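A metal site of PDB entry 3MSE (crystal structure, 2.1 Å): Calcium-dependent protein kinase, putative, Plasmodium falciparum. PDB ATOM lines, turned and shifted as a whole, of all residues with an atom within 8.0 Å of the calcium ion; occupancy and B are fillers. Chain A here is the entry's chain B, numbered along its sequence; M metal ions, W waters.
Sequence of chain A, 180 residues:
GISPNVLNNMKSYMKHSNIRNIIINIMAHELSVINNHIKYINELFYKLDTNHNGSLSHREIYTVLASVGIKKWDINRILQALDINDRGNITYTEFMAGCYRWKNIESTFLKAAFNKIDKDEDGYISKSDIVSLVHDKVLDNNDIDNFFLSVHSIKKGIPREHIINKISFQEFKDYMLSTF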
ATOM      1  N   PHE A  45      -8.271 -19.907   1.911  1.00  0.00           N
ATOM      2  CA  PHE A  45      -7.510 -18.706   1.577  1.00  0.00           C
ATOM      3  C   PHE A  45      -6.201 -19.039   0.867  1.00  0.00           C
ATOM      4  O   PHE A  45      -5.844 -18.400  -0.115  1.00  0.00           O
ATOM      5  CB  PHE A  45      -7.242 -17.881   2.855  1.00  0.00           C
ATOM      6  CG  PHE A  45      -6.510 -16.606   2.609  1.00  0.00           C
ATOM      7  CD1 PHE A  45      -7.204 -15.423   2.374  1.00  0.00           C
ATOM      8  CD2 PHE A  45      -5.111 -16.566   2.620  1.00  0.00           C
ATOM      9  CE1 PHE A  45      -6.538 -14.226   2.131  1.00  0.00           C
ATOM     10  CE2 PHE A  45      -4.431 -15.372   2.381  1.00  0.00           C
ATOM     11  CZ  PHE A  45      -5.156 -14.199   2.140  1.00  0.00           C
ATOM     12  N   TYR A  46      -5.490 -20.057   1.368  1.00  0.00           N
ATOM     13  CA  TYR A  46      -4.215 -20.476   0.814  1.00  0.00           C
ATOM     14  C   TYR A  46      -4.371 -20.967  -0.636  1.00  0.00           C
ATOM     15  O   TYR A  46      -3.558 -20.639  -1.492  1.00  0.00           O
ATOM     16  CB  TYR A  46      -3.566 -21.562   1.699  1.00  0.00           C
ATOM     17  CG  TYR A  46      -2.157 -21.964   1.270  1.00  0.00           C
ATOM     18  CD1 TYR A  46      -1.036 -21.289   1.764  1.00  0.00           C
ATOM     19  CD2 TYR A  46      -1.954 -23.025   0.370  1.00  0.00           C
ATOM     20  CE1 TYR A  46       0.251 -21.644   1.383  1.00  0.00           C
ATOM     21  CE2 TYR A  46      -0.658 -23.396  -0.027  1.00  0.00           C
ATOM     22  CZ  TYR A  46       0.432 -22.699   0.490  1.00  0.00           C
ATOM     23  OH  TYR A  46       1.705 -23.051   0.105  1.00  0.00           O
ATOM     24  N   LEU A  48      -6.843 -20.075  -2.763  1.00  0.00           N
ATOM     25  CA  LEU A  48      -7.232 -18.966  -3.639  1.00  0.00           C
ATOM     26  C   LEU A  48      -6.078 -18.042  -3.999  1.00  0.00           C
ATOM     27  O   LEU A  48      -6.039 -17.479  -5.091  1.00  0.00           O
ATOM     28  CB  LEU A  48      -8.374 -18.136  -3.051  1.00  0.00           C
ATOM     29  CG  LEU A  48      -9.679 -18.819  -2.622  1.00  0.00           C
ATOM     30  CD1 LEU A  48     -10.808 -17.811  -2.634  1.00  0.00           C
ATOM     31  CD2 LEU A  48      -9.993 -19.980  -3.533  1.00  0.00           C
ATOM     32  N   ASP A  49      -5.150 -17.916  -3.059  1.00  0.00           N
ATOM     33  CA  ASP A  49      -4.026 -17.002  -3.184  1.00  0.00           C
ATOM     34  C   ASP A  49      -2.945 -17.652  -4.049  1.00  0.00           C
ATOM     35  O   ASP A  49      -1.897 -18.080  -3.528  1.00  0.00           O
ATOM     36  CB  ASP A  49      -3.501 -16.687  -1.775  1.00  0.00           C
ATOM     37  CG  ASP A  49      -2.409 -15.647  -1.760  1.00  0.00           C
ATOM     38  OD1 ASP A  49      -2.295 -14.846  -2.706  1.00  0.00           O
ATOM     39  OD2 ASP A  49      -1.677 -15.638  -0.758  1.00  0.00           O
ATOM     40  N   THR A  50      -3.192 -17.714  -5.352  1.00  0.00           N
ATOM     41  CA  THR A  50      -2.339 -18.471  -6.271  1.00  0.00           C
ATOM     42  C   THR A  50      -0.971 -17.827  -6.526  1.00  0.00           C
ATOM     43  O   THR A  50      -0.064 -18.489  -7.021  1.00  0.00           O
ATOM     44  CB  THR A  50      -3.022 -18.766  -7.636  1.00  0.00           C
ATOM     45  OG1 THR A  50      -3.482 -17.531  -8.207  1.00  0.00           O
ATOM     46  CG2 THR A  50      -4.179 -19.740  -7.473  1.00  0.00           C
ATOM     47  N   ASN A  51      -0.810 -16.551  -6.183  1.00  0.00           N
ATOM     48  CA  ASN A  51       0.496 -15.906  -6.246  1.00  0.00           C
ATOM     49  C   ASN A  51       1.150 -15.819  -4.871  1.00  0.00           C
ATOM     50  O   ASN A  51       2.219 -15.245  -4.707  1.00  0.00           O
ATOM     51  CB  ASN A  51       0.424 -14.555  -6.946  1.00  0.00           C
ATOM     52  CG  ASN A  51      -0.396 -13.518  -6.177  1.00  0.00           C
ATOM     53  OD1 ASN A  51      -1.013 -13.829  -5.148  1.00  0.00           O
ATOM     54  ND2 ASN A  51      -0.404 -12.299  -6.682  1.00  0.00           N
ATOM     55  N   HIS A  52       0.493 -16.403  -3.873  1.00  0.00           N
ATOM     56  CA  HIS A  52       1.028 -16.448  -2.509  1.00  0.00           C
ATOM     57  C   HIS A  52       1.586 -15.094  -2.011  1.00  0.00           C
ATOM     58  O   HIS A  52       2.698 -15.034  -1.467  1.00  0.00           O
ATOM     59  CB  HIS A  52       2.073 -17.574  -2.378  1.00  0.00           C
ATOM     60  CG  HIS A  52       1.565 -18.934  -2.787  1.00  0.00           C
ATOM     61  ND1 HIS A  52       0.444 -19.510  -2.226  1.00  0.00           N
ATOM     62  CD2 HIS A  52       2.032 -19.819  -3.702  1.00  0.00           C
ATOM     63  CE1 HIS A  52       0.236 -20.689  -2.777  1.00  0.00           C
ATOM     64  NE2 HIS A  52       1.185 -20.907  -3.667  1.00  0.00           N
ATOM     65  N   ASN A  53       0.823 -14.023  -2.226  1.00  0.00           N
ATOM     66  CA  ASN A  53       1.166 -12.686  -1.728  1.00  0.00           C
ATOM     67  C   ASN A  53       0.324 -12.301  -0.487  1.00  0.00           C
ATOM     68  O   ASN A  53       0.299 -11.150  -0.069  1.00  0.00           O
ATOM     69  CB  ASN A  53       0.972 -11.640  -2.847  1.00  0.00           C
ATOM     70  CG  ASN A  53      -0.478 -11.385  -3.154  1.00  0.00           C
ATOM     71  OD1 ASN A  53      -1.333 -12.080  -2.621  1.00  0.00           O
ATOM     72  ND2 ASN A  53      -0.763 -10.384  -3.985  1.00  0.00           N
ATOM     73  N   GLY A  54      -0.397 -13.272   0.084  1.00  0.00           N
ATOM     74  CA  GLY A  54      -1.082 -13.064   1.342  1.00  0.00           C
ATOM     75  C   GLY A  54      -2.368 -12.260   1.265  1.00  0.00           C
ATOM     76  O   GLY A  54      -2.964 -11.943   2.292  1.00  0.00           O
ATOM     77  N   SER A  55      -2.801 -11.919   0.055  1.00  0.00           N
ATOM     78  CA  SER A  55      -4.091 -11.289  -0.130  1.00  0.00           C
ATOM     79  C   SER A  55      -4.785 -11.807  -1.402  1.00  0.00           C
ATOM     80  O   SER A  55      -4.144 -12.450  -2.249  1.00  0.00           O
ATOM     81  CB  SER A  55      -3.957  -9.772  -0.162  1.00  0.00           C
ATOM     82  OG  SER A  55      -3.364  -9.378  -1.362  1.00  0.00           O
ATOM     83  N   LEU A  56      -6.086 -11.535  -1.531  1.00  0.00           N
ATOM     84  CA  LEU A  56      -6.889 -12.072  -2.641  1.00  0.00           C
ATOM     85  C   LEU A  56      -7.341 -11.007  -3.602  1.00  0.00           C
ATOM     86  O   LEU A  56      -8.024 -10.065  -3.215  1.00  0.00           O
ATOM     87  CB  LEU A  56      -8.125 -12.824  -2.113  1.00  0.00           C
ATOM     88  CG  LEU A  56      -7.892 -14.047  -1.230  1.00  0.00           C
ATOM     89  CD1 LEU A  56      -9.209 -14.754  -0.915  1.00  0.00           C
ATOM     90  CD2 LEU A  56      -6.901 -15.011  -1.878  1.00  0.00           C
ATOM     91  N   SER A  57      -6.973 -11.141  -4.876  1.00  0.00           N
ATOM     92  CA  SER A  57      -7.502 -10.233  -5.880  1.00  0.00           C
ATOM     93  C   SER A  57      -8.946 -10.624  -6.243  1.00  0.00           C
ATOM     94  O   SER A  57      -9.395 -11.712  -5.878  1.00  0.00           O
ATOM     95  CB  SER A  57      -6.630 -10.227  -7.139  1.00  0.00           C
ATOM     96  OG  SER A  57      -6.771 -11.431  -7.870  1.00  0.00           O
ATOM     97  N   ARG A  59     -10.013 -11.378  -9.267  1.00  0.00           N
ATOM     98  CA  ARG A  59      -9.859 -12.528 -10.174  1.00  0.00           C
ATOM     99  C   ARG A  59      -9.596 -13.837  -9.446  1.00  0.00           C
ATOM    100  O   ARG A  59     -10.216 -14.862  -9.768  1.00  0.00           O
ATOM    101  CB  ARG A  59      -8.737 -12.257 -11.189  1.00  0.00           C
ATOM    102  CG  ARG A  59      -8.415 -13.460 -12.069  1.00  0.00           C
ATOM    103  CD  ARG A  59      -7.125 -13.232 -12.858  1.00  0.00           C
ATOM    104  NE  ARG A  59      -5.965 -13.157 -11.960  1.00  0.00           N
ATOM    105  CZ  ARG A  59      -5.569 -14.142 -11.160  1.00  0.00           C
ATOM    106  NH1 ARG A  59      -6.239 -15.299 -11.115  1.00  0.00           N
ATOM    107  NH2 ARG A  59      -4.497 -13.965 -10.400  1.00  0.00           N
ATOM    108  N   GLU A  60      -8.691 -13.828  -8.470  1.00  0.00           N
ATOM    109  CA  GLU A  60      -8.385 -15.048  -7.689  1.00  0.00           C
ATOM    110  C   GLU A  60      -9.638 -15.689  -7.083  1.00  0.00           C
ATOM    111  O   GLU A  60      -9.776 -16.919  -7.067  1.00  0.00           O
ATOM    112  CB  GLU A  60      -7.361 -14.790  -6.579  1.00  0.00           C
ATOM    113  CG  GLU A  60      -5.913 -14.587  -7.088  1.00  0.00           C
ATOM    114  CD  GLU A  60      -4.920 -14.225  -5.970  1.00  0.00           C
ATOM    115  OE1 GLU A  60      -3.719 -14.500  -6.137  1.00  0.00           O
ATOM    116  OE2 GLU A  60      -5.335 -13.706  -4.906  1.00  0.00           O
ATOM    117  N   ASN A  89      -7.850  -5.580  -3.548  1.00  0.00           N
ATOM    118  CA  ASN A  89      -7.089  -6.601  -2.849  1.00  0.00           C
ATOM    119  C   ASN A  89      -7.865  -6.863  -1.556  1.00  0.00           C
ATOM    120  O   ASN A  89      -8.251  -5.919  -0.854  1.00  0.00           O
ATOM    121  CB  ASN A  89      -5.656  -6.108  -2.520  1.00  0.00           C
ATOM    122  CG  ASN A  89      -4.831  -5.827  -3.783  1.00  0.00           C
ATOM    123  OD1 ASN A  89      -4.249  -6.740  -4.377  1.00  0.00           O
ATOM    124  ND2 ASN A  89      -4.798  -4.565  -4.211  1.00  0.00           N
ATOM    125  N   ILE A  90      -8.124  -8.131  -1.271  1.00  0.00           N
ATOM    126  CA  ILE A  90      -8.931  -8.504  -0.123  1.00  0.00           C
ATOM    127  C   ILE A  90      -8.069  -9.223   0.877  1.00  0.00           C
ATOM    128  O   ILE A  90      -7.376 -10.193   0.539  1.00  0.00           O
ATOM    129  CB  ILE A  90     -10.133  -9.387  -0.556  1.00  0.00           C
ATOM    130  CG1 ILE A  90     -11.160  -8.509  -1.284  1.00  0.00           C
ATOM    131  CG2 ILE A  90     -10.754 -10.078   0.653  1.00  0.00           C
ATOM    132  CD1 ILE A  90     -11.807  -9.180  -2.451  1.00  0.00           C
HETATM  133 CA    CA M   1      -2.935 -13.304  -3.992  1.00  0.00          CA
HETATM  134  O   HOH W   1      -3.179 -11.860  -5.159  1.00  0.00           O
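Water W1 bridges ND2 of Asn 53 (3.1 Å) and ND2 of Asn 51 (3.2 Å).
The calcium ion is bound by water W1, OD1 of Asp 49, O of Ser 55, OD1 of Asn 51, OD1 of Asn 53, OE1 of Glu 60 and OE2 of Glu 60. The calcium ion has seven donor atoms within binding distance.
The backbone carbonyl oxygen (O) of Asp 49 lies within hydrogen-bond range of a ring nitrogen (ND1) of His 52 (3.0 Å). N of Gly 54 is in hydrogen-bond range of OD2 of Asp 49. OE1 of Glu 60 sits close to N of Thr 50, at 3.4 Å. The side-chain hydroxyl (OG) of Ser 57 sits at hydrogen-bond distance from the backbone NH (N) of Glu 60 (3.1 Å).
Within 4 Å of the calcium ion: Asp 49, Asn 51, Asn 53, Ser 55 and Glu 60. The nearest printed residue that does not touch the calcium ion is Leu 56 (4.4 Å).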
